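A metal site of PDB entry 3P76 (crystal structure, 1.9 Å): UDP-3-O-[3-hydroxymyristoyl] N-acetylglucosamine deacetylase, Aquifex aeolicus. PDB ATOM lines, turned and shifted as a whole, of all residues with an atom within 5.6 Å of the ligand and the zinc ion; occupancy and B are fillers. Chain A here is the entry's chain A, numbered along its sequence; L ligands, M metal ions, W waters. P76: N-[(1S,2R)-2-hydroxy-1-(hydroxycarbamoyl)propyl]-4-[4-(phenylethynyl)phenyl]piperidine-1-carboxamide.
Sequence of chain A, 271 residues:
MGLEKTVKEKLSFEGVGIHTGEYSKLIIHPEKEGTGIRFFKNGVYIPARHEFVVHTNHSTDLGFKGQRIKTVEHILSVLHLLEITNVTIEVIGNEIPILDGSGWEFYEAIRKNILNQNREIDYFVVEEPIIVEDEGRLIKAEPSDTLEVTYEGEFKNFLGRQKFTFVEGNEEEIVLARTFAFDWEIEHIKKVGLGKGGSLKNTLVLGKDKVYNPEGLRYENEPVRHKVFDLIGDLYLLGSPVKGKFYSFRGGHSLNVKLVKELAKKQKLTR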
ATOM      1  N   ILE A  18       0.393 -23.147 -16.070  1.00  0.00           N
ATOM      2  CA  ILE A  18      -0.301 -22.600 -14.893  1.00  0.00           C
ATOM      3  C   ILE A  18      -1.507 -21.700 -15.216  1.00  0.00           C
ATOM      4  O   ILE A  18      -2.512 -21.728 -14.502  1.00  0.00           O
ATOM      5  CB  ILE A  18       0.658 -21.941 -13.878  1.00  0.00           C
ATOM      6  CG1 ILE A  18       0.059 -21.960 -12.445  1.00  0.00           C
ATOM      7  CG2 ILE A  18       1.099 -20.532 -14.317  1.00  0.00           C
ATOM      8  CD1 ILE A  18       1.040 -21.823 -11.362  1.00  0.00           C
ATOM      9  N   HIS A  19      -1.387 -20.879 -16.273  1.00  0.00           N
ATOM     10  CA  HIS A  19      -2.479 -19.956 -16.610  1.00  0.00           C
ATOM     11  C   HIS A  19      -3.539 -20.520 -17.518  1.00  0.00           C
ATOM     12  O   HIS A  19      -4.722 -20.357 -17.234  1.00  0.00           O
ATOM     13  CB  HIS A  19      -1.920 -18.615 -17.111  1.00  0.00           C
ATOM     14  CG  HIS A  19      -1.263 -17.814 -16.040  1.00  0.00           C
ATOM     15  ND1 HIS A  19      -1.946 -17.418 -14.903  1.00  0.00           N
ATOM     16  CD2 HIS A  19       0.010 -17.367 -15.954  1.00  0.00           C
ATOM     17  CE1 HIS A  19      -1.075 -16.765 -14.157  1.00  0.00           C
ATOM     18  NE2 HIS A  19       0.119 -16.716 -14.739  1.00  0.00           N
ATOM     19  N   HIS A  58       0.604 -11.115 -13.914  1.00  0.00           N
ATOM     20  CA  HIS A  58       0.706 -12.478 -13.340  1.00  0.00           C
ATOM     21  C   HIS A  58       1.625 -13.434 -14.106  1.00  0.00           C
ATOM     22  O   HIS A  58       1.853 -14.556 -13.650  1.00  0.00           O
ATOM     23  CB  HIS A  58      -0.678 -13.096 -13.007  1.00  0.00           C
ATOM     24  CG  HIS A  58      -1.537 -12.184 -12.182  1.00  0.00           C
ATOM     25  ND1 HIS A  58      -1.311 -12.012 -10.835  1.00  0.00           N
ATOM     26  CD2 HIS A  58      -2.575 -11.398 -12.569  1.00  0.00           C
ATOM     27  CE1 HIS A  58      -2.212 -11.118 -10.432  1.00  0.00           C
ATOM     28  NE2 HIS A  58      -3.005 -10.738 -11.434  1.00  0.00           N
ATOM     29  N   SER A  59       2.185 -12.967 -15.227  1.00  0.00           N
ATOM     30  CA  SER A  59       3.149 -13.704 -16.067  1.00  0.00           C
ATOM     31  C   SER A  59       3.700 -12.770 -17.113  1.00  0.00           C
ATOM     32  O   SER A  59       3.081 -11.768 -17.441  1.00  0.00           O
ATOM     33  CB  SER A  59       2.498 -14.912 -16.737  1.00  0.00           C
ATOM     34  OG  SER A  59       1.578 -14.550 -17.751  1.00  0.00           O
ATOM     35  N   THR A  71       3.858 -17.169 -20.064  1.00  0.00           N
ATOM     36  CA  THR A  71       4.715 -17.580 -18.948  1.00  0.00           C
ATOM     37  C   THR A  71       6.129 -18.009 -19.361  1.00  0.00           C
ATOM     38  O   THR A  71       6.554 -19.128 -19.091  1.00  0.00           O
ATOM     39  CB  THR A  71       3.936 -18.617 -18.077  1.00  0.00           C
ATOM     40  OG1 THR A  71       2.544 -18.253 -18.086  1.00  0.00           O
ATOM     41  CG2 THR A  71       4.450 -18.734 -16.651  1.00  0.00           C
ATOM     42  N   GLU A  73       8.904 -16.500 -18.176  1.00  0.00           N
ATOM     43  CA  GLU A  73       9.841 -16.116 -17.100  1.00  0.00           C
ATOM     44  C   GLU A  73      10.730 -17.187 -16.455  1.00  0.00           C
ATOM     45  O   GLU A  73      11.902 -16.927 -16.222  1.00  0.00           O
ATOM     46  CB  GLU A  73       9.167 -15.186 -16.061  1.00  0.00           C
ATOM     47  CG  GLU A  73       8.018 -15.843 -15.325  1.00  0.00           C
ATOM     48  CD  GLU A  73       6.616 -15.658 -15.903  1.00  0.00           C
ATOM     49  OE1 GLU A  73       6.484 -15.442 -17.120  1.00  0.00           O
ATOM     50  OE2 GLU A  73       5.650 -15.757 -15.116  1.00  0.00           O
ATOM     51  N   HIS A  74      10.177 -18.377 -16.171  1.00  0.00           N
ATOM     52  CA  HIS A  74      10.921 -19.451 -15.494  1.00  0.00           C
ATOM     53  C   HIS A  74      11.973 -20.089 -16.385  1.00  0.00           C
ATOM     54  O   HIS A  74      13.114 -20.247 -15.952  1.00  0.00           O
ATOM     55  CB  HIS A  74       9.961 -20.495 -14.870  1.00  0.00           C
ATOM     56  CG  HIS A  74       8.941 -19.919 -13.926  1.00  0.00           C
ATOM     57  ND1 HIS A  74       7.890 -20.682 -13.464  1.00  0.00           N
ATOM     58  CD2 HIS A  74       8.870 -18.683 -13.369  1.00  0.00           C
ATOM     59  CE1 HIS A  74       7.203 -19.895 -12.643  1.00  0.00           C
ATOM     60  NE2 HIS A  74       7.747 -18.666 -12.588  1.00  0.00           N
ATOM     61  N   GLY A 101       6.418 -25.699 -10.361  1.00  0.00           N
ATOM     62  CA  GLY A 101       6.324 -24.285 -10.011  1.00  0.00           C
ATOM     63  C   GLY A 101       7.671 -23.593  -9.912  1.00  0.00           C
ATOM     64  O   GLY A 101       7.740 -22.378  -9.741  1.00  0.00           O
ATOM     65  N   THR A 179       6.571 -20.801  -7.569  1.00  0.00           N
ATOM     66  CA  THR A 179       5.579 -19.743  -7.733  1.00  0.00           C
ATOM     67  C   THR A 179       4.593 -19.855  -6.546  1.00  0.00           C
ATOM     68  O   THR A 179       4.429 -20.939  -5.959  1.00  0.00           O
ATOM     69  CB  THR A 179       4.901 -19.796  -9.113  1.00  0.00           C
ATOM     70  OG1 THR A 179       4.003 -18.685  -9.203  1.00  0.00           O
ATOM     71  CG2 THR A 179       4.158 -21.081  -9.367  1.00  0.00           C
ATOM     72  N   PHE A 180       4.024 -18.729  -6.158  1.00  0.00           N
ATOM     73  CA  PHE A 180       3.144 -18.693  -4.999  1.00  0.00           C
ATOM     74  C   PHE A 180       1.920 -17.848  -5.250  1.00  0.00           C
ATOM     75  O   PHE A 180       1.891 -17.050  -6.197  1.00  0.00           O
ATOM     76  CB  PHE A 180       3.913 -18.222  -3.744  1.00  0.00           C
ATOM     77  CG  PHE A 180       4.436 -16.803  -3.839  1.00  0.00           C
ATOM     78  CD1 PHE A 180       3.749 -15.756  -3.253  1.00  0.00           C
ATOM     79  CD2 PHE A 180       5.647 -16.524  -4.486  1.00  0.00           C
ATOM     80  CE1 PHE A 180       4.230 -14.441  -3.327  1.00  0.00           C
ATOM     81  CE2 PHE A 180       6.103 -15.208  -4.603  1.00  0.00           C
ATOM     82  CZ  PHE A 180       5.407 -14.180  -4.009  1.00  0.00           C
ATOM     83  N   ALA A 181       0.901 -18.016  -4.408  1.00  0.00           N
ATOM     84  CA  ALA A 181      -0.349 -17.274  -4.480  1.00  0.00           C
ATOM     85  C   ALA A 181      -0.961 -17.137  -3.103  1.00  0.00           C
ATOM     86  O   ALA A 181      -0.743 -17.978  -2.219  1.00  0.00           O
ATOM     87  CB  ALA A 181      -1.335 -17.966  -5.416  1.00  0.00           C
ATOM     88  N   ILE A 186      -6.860 -15.441  -5.316  1.00  0.00           N
ATOM     89  CA  ILE A 186      -7.201 -16.474  -6.304  1.00  0.00           C
ATOM     90  C   ILE A 186      -8.490 -16.207  -7.093  1.00  0.00           C
ATOM     91  O   ILE A 186      -8.477 -16.346  -8.307  1.00  0.00           O
ATOM     92  CB  ILE A 186      -7.098 -17.926  -5.721  1.00  0.00           C
ATOM     93  CG1 ILE A 186      -5.644 -18.232  -5.278  1.00  0.00           C
ATOM     94  CG2 ILE A 186      -7.607 -18.980  -6.741  1.00  0.00           C
ATOM     95  CD1 ILE A 186      -5.496 -19.457  -4.360  1.00  0.00           C
ATOM     96  N   ILE A 189      -7.831 -13.735  -9.852  1.00  0.00           N
ATOM     97  CA  ILE A 189      -6.976 -14.341 -10.879  1.00  0.00           C
ATOM     98  C   ILE A 189      -7.811 -15.253 -11.814  1.00  0.00           C
ATOM     99  O   ILE A 189      -7.673 -15.136 -13.032  1.00  0.00           O
ATOM    100  CB  ILE A 189      -5.729 -15.038 -10.245  1.00  0.00           C
ATOM    101  CG1 ILE A 189      -4.814 -13.976  -9.580  1.00  0.00           C
ATOM    102  CG2 ILE A 189      -4.950 -15.880 -11.274  1.00  0.00           C
ATOM    103  CD1 ILE A 189      -3.826 -14.477  -8.504  1.00  0.00           C
ATOM    104  N   LYS A 190      -8.713 -16.074 -11.246  1.00  0.00           N
ATOM    105  CA  LYS A 190      -9.597 -16.967 -11.994  1.00  0.00           C
ATOM    106  C   LYS A 190     -10.620 -16.151 -12.807  1.00  0.00           C
ATOM    107  O   LYS A 190     -10.900 -16.482 -13.963  1.00  0.00           O
ATOM    108  CB  LYS A 190     -10.337 -17.954 -11.071  1.00  0.00           C
ATOM    109  CG  LYS A 190      -9.441 -18.876 -10.244  1.00  0.00           C
ATOM    110  CD  LYS A 190      -8.890 -20.099 -10.975  1.00  0.00           C
ATOM    111  CE  LYS A 190      -8.487 -21.157  -9.972  1.00  0.00           C
ATOM    112  NZ  LYS A 190      -7.532 -22.150 -10.530  1.00  0.00           N
ATOM    113  N   GLY A 195      -4.706 -18.388 -14.093  1.00  0.00           N
ATOM    114  CA  GLY A 195      -4.458 -19.430 -13.098  1.00  0.00           C
ATOM    115  C   GLY A 195      -5.258 -20.719 -13.243  1.00  0.00           C
ATOM    116  O   GLY A 195      -5.482 -21.396 -12.246  1.00  0.00           O
ATOM    117  N   GLY A 198      -3.355 -23.846 -12.007  1.00  0.00           N
ATOM    118  CA  GLY A 198      -2.809 -23.670 -10.666  1.00  0.00           C
ATOM    119  C   GLY A 198      -3.391 -24.659  -9.679  1.00  0.00           C
ATOM    120  O   GLY A 198      -4.601 -24.876  -9.669  1.00  0.00           O
ATOM    121  N   SER A 199      -2.517 -25.283  -8.878  1.00  0.00           N
ATOM    122  CA  SER A 199      -2.930 -26.261  -7.869  1.00  0.00           C
ATOM    123  C   SER A 199      -1.853 -26.354  -6.800  1.00  0.00           C
ATOM    124  O   SER A 199      -0.801 -25.741  -6.944  1.00  0.00           O
ATOM    125  CB  SER A 199      -3.142 -27.632  -8.523  1.00  0.00           C
ATOM    126  OG  SER A 199      -1.919 -28.295  -8.800  1.00  0.00           O
ATOM    127  N   LEU A 200      -2.101 -27.159  -5.749  1.00  0.00           N
ATOM    128  CA  LEU A 200      -1.122 -27.376  -4.684  1.00  0.00           C
ATOM    129  C   LEU A 200       0.081 -28.191  -5.161  1.00  0.00           C
ATOM    130  O   LEU A 200       1.069 -28.292  -4.449  1.00  0.00           O
ATOM    131  CB  LEU A 200      -1.788 -27.997  -3.440  1.00  0.00           C
ATOM    132  CG  LEU A 200      -2.844 -27.140  -2.725  1.00  0.00           C
ATOM    133  CD1 LEU A 200      -3.436 -27.875  -1.522  1.00  0.00           C
ATOM    134  CD2 LEU A 200      -2.270 -25.792  -2.289  1.00  0.00           C
ATOM    135  N   ASN A 202       1.771 -27.452  -8.042  1.00  0.00           N
ATOM    136  CA  ASN A 202       2.681 -26.544  -8.736  1.00  0.00           C
ATOM    137  C   ASN A 202       2.760 -25.140  -8.114  1.00  0.00           C
ATOM    138  O   ASN A 202       3.488 -24.286  -8.630  1.00  0.00           O
ATOM    139  CB  ASN A 202       2.299 -26.447 -10.232  1.00  0.00           C
ATOM    140  CG  ASN A 202       0.860 -26.055 -10.501  1.00  0.00           C
ATOM    141  OD1 ASN A 202       0.306 -25.146  -9.877  1.00  0.00           O
ATOM    142  ND2 ASN A 202       0.238 -26.684 -11.479  1.00  0.00           N
ATOM    143  N   THR A 203       2.004 -24.875  -7.042  1.00  0.00           N
ATOM    144  CA  THR A 203       1.990 -23.554  -6.396  1.00  0.00           C
ATOM    145  C   THR A 203       2.002 -23.650  -4.890  1.00  0.00           C
ATOM    146  O   THR A 203       1.276 -24.464  -4.304  1.00  0.00           O
ATOM    147  CB  THR A 203       0.759 -22.740  -6.865  1.00  0.00           C
ATOM    148  OG1 THR A 203       0.713 -22.689  -8.289  1.00  0.00           O
ATOM    149  CG2 THR A 203       0.727 -21.319  -6.289  1.00  0.00           C
ATOM    150  N   VAL A 205       0.553 -22.196  -1.902  1.00  0.00           N
ATOM    151  CA  VAL A 205      -0.631 -21.404  -1.591  1.00  0.00           C
ATOM    152  C   VAL A 205      -0.679 -21.071  -0.095  1.00  0.00           C
ATOM    153  O   VAL A 205      -0.636 -21.962   0.756  1.00  0.00           O
ATOM    154  CB  VAL A 205      -1.943 -22.023  -2.127  1.00  0.00           C
ATOM    155  CG1 VAL A 205      -3.137 -21.131  -1.785  1.00  0.00           C
ATOM    156  CG2 VAL A 205      -1.853 -22.259  -3.636  1.00  0.00           C
ATOM    157  N   TYR A 212      -1.386 -23.916   2.809  1.00  0.00           N
ATOM    158  CA  TYR A 212      -2.275 -24.946   2.264  1.00  0.00           C
ATOM    159  C   TYR A 212      -1.535 -26.236   1.891  1.00  0.00           C
ATOM    160  O   TYR A 212      -2.070 -27.323   2.095  1.00  0.00           O
ATOM    161  CB  TYR A 212      -3.026 -24.406   1.028  1.00  0.00           C
ATOM    162  CG  TYR A 212      -4.177 -23.475   1.354  1.00  0.00           C
ATOM    163  CD1 TYR A 212      -3.952 -22.155   1.713  1.00  0.00           C
ATOM    164  CD2 TYR A 212      -5.503 -23.903   1.226  1.00  0.00           C
ATOM    165  CE1 TYR A 212      -5.001 -21.294   2.017  1.00  0.00           C
ATOM    166  CE2 TYR A 212      -6.566 -23.045   1.512  1.00  0.00           C
ATOM    167  CZ  TYR A 212      -6.314 -21.747   1.894  1.00  0.00           C
ATOM    168  OH  TYR A 212      -7.360 -20.887   2.139  1.00  0.00           O
ATOM    169  N   HIS A 226      11.611 -16.873  -5.013  1.00  0.00           N
ATOM    170  CA  HIS A 226      10.927 -17.043  -6.299  1.00  0.00           C
ATOM    171  C   HIS A 226      10.837 -15.725  -7.047  1.00  0.00           C
ATOM    172  O   HIS A 226      10.990 -15.707  -8.264  1.00  0.00           O
ATOM    173  CB  HIS A 226       9.528 -17.661  -6.167  1.00  0.00           C
ATOM    174  CG  HIS A 226       8.935 -17.934  -7.524  1.00  0.00           C
ATOM    175  ND1 HIS A 226       9.337 -19.023  -8.269  1.00  0.00           N
ATOM    176  CD2 HIS A 226       8.107 -17.166  -8.274  1.00  0.00           C
ATOM    177  CE1 HIS A 226       8.713 -18.926  -9.436  1.00  0.00           C
ATOM    178  NE2 HIS A 226       7.954 -17.825  -9.485  1.00  0.00           N
ATOM    179  N   LYS A 227      10.580 -14.633  -6.333  1.00  0.00           N
ATOM    180  CA  LYS A 227      10.502 -13.304  -6.941  1.00  0.00           C
ATOM    181  C   LYS A 227      11.862 -12.875  -7.526  1.00  0.00           C
ATOM    182  O   LYS A 227      11.899 -12.227  -8.578  1.00  0.00           O
ATOM    183  CB  LYS A 227       9.976 -12.298  -5.915  1.00  0.00           C
ATOM    184  CG  LYS A 227       8.451 -12.379  -5.685  1.00  0.00           C
ATOM    185  CD  LYS A 227       7.658 -11.737  -6.834  1.00  0.00           C
ATOM    186  CE  LYS A 227       6.203 -11.534  -6.511  1.00  0.00           C
ATOM    187  NZ  LYS A 227       5.479 -10.899  -7.649  1.00  0.00           N
ATOM    188  N   PHE A 229      14.093 -15.101  -8.740  1.00  0.00           N
ATOM    189  CA  PHE A 229      14.102 -15.996  -9.896  1.00  0.00           C
ATOM    190  C   PHE A 229      13.261 -15.403 -11.070  1.00  0.00           C
ATOM    191  O   PHE A 229      13.728 -15.386 -12.213  1.00  0.00           O
ATOM    192  CB  PHE A 229      13.625 -17.383  -9.452  1.00  0.00           C
ATOM    193  CG  PHE A 229      13.503 -18.423 -10.534  1.00  0.00           C
ATOM    194  CD1 PHE A 229      14.620 -19.083 -11.030  1.00  0.00           C
ATOM    195  CD2 PHE A 229      12.258 -18.774 -11.050  1.00  0.00           C
ATOM    196  CE1 PHE A 229      14.507 -20.029 -12.045  1.00  0.00           C
ATOM    197  CE2 PHE A 229      12.136 -19.729 -12.047  1.00  0.00           C
ATOM    198  CZ  PHE A 229      13.261 -20.353 -12.548  1.00  0.00           C
ATOM    199  N   ASP A 230      12.086 -14.847 -10.755  1.00  0.00           N
ATOM    200  CA  ASP A 230      11.211 -14.188 -11.749  1.00  0.00           C
ATOM    201  C   ASP A 230      11.903 -12.992 -12.405  1.00  0.00           C
ATOM    202  O   ASP A 230      11.871 -12.860 -13.630  1.00  0.00           O
ATOM    203  CB  ASP A 230       9.900 -13.707 -11.091  1.00  0.00           C
ATOM    204  CG  ASP A 230       8.842 -14.773 -10.909  1.00  0.00           C
ATOM    205  OD1 ASP A 230       8.967 -15.852 -11.546  1.00  0.00           O
ATOM    206  OD2 ASP A 230       7.842 -14.500 -10.202  1.00  0.00           O
ATOM    207  N   HIS A 253       6.214  -8.395 -12.688  1.00  0.00           N
ATOM    208  CA  HIS A 253       6.580  -8.429 -14.117  1.00  0.00           C
ATOM    209  C   HIS A 253       6.431  -7.089 -14.831  1.00  0.00           C
ATOM    210  O   HIS A 253       7.297  -6.744 -15.630  1.00  0.00           O
ATOM    211  CB  HIS A 253       5.835  -9.528 -14.882  1.00  0.00           C
ATOM    212  CG  HIS A 253       6.028 -10.892 -14.289  1.00  0.00           C
ATOM    213  ND1 HIS A 253       7.274 -11.510 -14.291  1.00  0.00           N
ATOM    214  CD2 HIS A 253       5.131 -11.712 -13.691  1.00  0.00           C
ATOM    215  CE1 HIS A 253       7.083 -12.683 -13.697  1.00  0.00           C
ATOM    216  NE2 HIS A 253       5.825 -12.834 -13.309  1.00  0.00           N
HETATM  217  N1  P76 L   1       2.618 -16.110 -10.273  1.00  0.00           N
HETATM  218  C2  P76 L   1       3.714 -15.172 -10.168  1.00  0.00           C
HETATM  219  C3  P76 L   1       4.844 -15.817 -10.947  1.00  0.00           C
HETATM  220  O4  P76 L   1       5.437 -16.830 -10.560  1.00  0.00           O
HETATM  221  N5  P76 L   1       5.105 -15.112 -12.086  1.00  0.00           N
HETATM  222  O6  P76 L   1       6.156 -15.700 -12.768  1.00  0.00           O
HETATM  223  C7  P76 L   1       1.282 -15.671 -10.074  1.00  0.00           C
HETATM  224  O8  P76 L   1       0.990 -14.482  -9.806  1.00  0.00           O
HETATM  225  N9  P76 L   1       0.322 -16.667 -10.201  1.00  0.00           N
HETATM  226  C10 P76 L   1       0.594 -18.069 -10.559  1.00  0.00           C
HETATM  227  C11 P76 L   1      -0.179 -19.009  -9.675  1.00  0.00           C
HETATM  228  C12 P76 L   1      -1.685 -18.790  -9.867  1.00  0.00           C
HETATM  229  C13 P76 L   1      -1.960 -17.368  -9.361  1.00  0.00           C
HETATM  230  C14 P76 L   1      -1.103 -16.295 -10.032  1.00  0.00           C
HETATM  231  C15 P76 L   1      -2.538 -19.758  -9.060  1.00  0.00           C
HETATM  232  C16 P76 L   1      -3.960 -19.658  -9.010  1.00  0.00           C
HETATM  233  C17 P76 L   1      -4.719 -20.570  -8.241  1.00  0.00           C
HETATM  234  C18 P76 L   1      -4.048 -21.588  -7.525  1.00  0.00           C
HETATM  235  C19 P76 L   1      -2.670 -21.711  -7.557  1.00  0.00           C
HETATM  236  C20 P76 L   1      -1.947 -20.818  -8.320  1.00  0.00           C
HETATM  237  C21 P76 L   1      -4.683 -22.526  -6.702  1.00  0.00           C
HETATM  238  C22 P76 L   1      -5.125 -23.208  -5.836  1.00  0.00           C
HETATM  239  C23 P76 L   1      -5.648 -24.011  -4.799  1.00  0.00           C
HETATM  240  C24 P76 L   1      -5.991 -23.351  -3.587  1.00  0.00           C
HETATM  241  C25 P76 L   1      -6.532 -24.090  -2.514  1.00  0.00           C
HETATM  242  C26 P76 L   1      -6.714 -25.483  -2.658  1.00  0.00           C
HETATM  243  C27 P76 L   1      -6.363 -26.130  -3.871  1.00  0.00           C
HETATM  244  C28 P76 L   1      -5.829 -25.389  -4.957  1.00  0.00           C
HETATM  245  C29 P76 L   1       4.103 -14.715  -8.749  1.00  0.00           C
HETATM  246  C30 P76 L   1       4.424 -15.845  -7.782  1.00  0.00           C
HETATM  247  O31 P76 L   1       5.266 -13.879  -8.887  1.00  0.00           O
HETATM  248 ZN    ZN M   1       7.365 -17.024 -11.262  1.00  0.00          ZN
HETATM  249  O   HOH W   1       3.198 -16.878 -14.013  1.00  0.00           O
HETATM  250  O   HOH W   2       1.051 -14.320  -6.433  1.00  0.00           O
HETATM  251  O   HOH W   3       3.742 -18.805 -12.244  1.00  0.00           O
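The side-chain carboxylate (OE2) of Glu 73 is in hydrogen-bond range of a nitrogen (N5) of the ligand (3.1 Å). NE2 of His 253 sits at hydrogen-bond distance from N5 of the ligand, 2.7 Å away. A nitrogen (N1) of the ligand is in hydrogen-bond range of the side-chain hydroxyl of Thr 179. O31 of the ligand sits at hydrogen-bond distance from NZ of Lys 227 (3.2 Å).
The backbone NH (N) of Thr 179 sits at hydrogen-bond distance from a ring nitrogen (ND1) of His 226 (3.4 Å). OE2 of Glu 73 is in hydrogen-bond range of NE2 of His 253. The backbone NH of Thr 179 sits at hydrogen-bond distance from the backbone carbonyl oxygen of Gly 101. The side-chain amide oxygen (OD1) of Asn 202 sits at hydrogen-bond distance from the side-chain hydroxyl (OG1) of Thr 203 (3.0 Å). A ring nitrogen (NE2) of His 19 is in hydrogen-bond range of the backbone carbonyl oxygen of His 58 (3.0 Å). The side-chain amide oxygen of Asn 202 sits at hydrogen-bond distance from the backbone NH of Ser 199 (3.0 Å). N of Tyr 212 is in hydrogen-bond range of O of Val 205 (2.9 Å). NZ of Lys 190 lies within hydrogen-bond range of O of Gly 195, at 2.8 Å.
CD1 of Ile 18 touches C11 of the ligand, at 3.5 Å. His 58 touches the ligand (ND1 to O8, 3.5 Å). O of Phe 180 touches C30 of the ligand, 3.2 Å away. Ile 186 touches the ligand (CG2 to C17, 3.6 Å). Ile 189 touches the ligand. Lys 190 touches the ligand (NZ to C17, 3.96 Å). O of Gly 195 touches C16 of the ligand (3.98 Å). Gly 198 touches the ligand. Ser 199 touches the ligand. Leu 200 touches the ligand (CG to C27, 3.8 Å). Thr 203 touches the ligand (OG1 to C20, 3.3 Å). Tyr 212 touches the ligand. Of the 27 residues printed, 19 come within 4 Å of the ligand. The nearest printed residue that does not touch the ligand is Ala 181 (4.04 Å).
Of the 27 residues printed, 3 come within 4 Å of the zinc ion. The nearest printed residue that does not touch the zinc ion is Thr 179 (4.3 Å).
The zinc ion is bound by OD1 of Asp 230 (2.0 Å), NE2 of His 226 (2.0 Å), O4 of the ligand (2.1 Å), NE2 of His 74 (2.1 Å) and O6 of the ligand (2.3 Å). Slightly farther from the zinc ion lies the side-chain carboxylate (OD2) of Asp 230 (2.8 Å).
Water W1 lies within hydrogen-bond range of O of His 58 (2.7 Å), OE2 of Glu 73 (2.9 Å), NE2 of His 19 (3.2 Å) and N5 of the ligand (3.2 Å). Water W2 bridges the backbone carbonyl oxygen (O) of Phe 180 (2.9 Å) and an oxygen (O8) of the ligand (3.4 Å).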
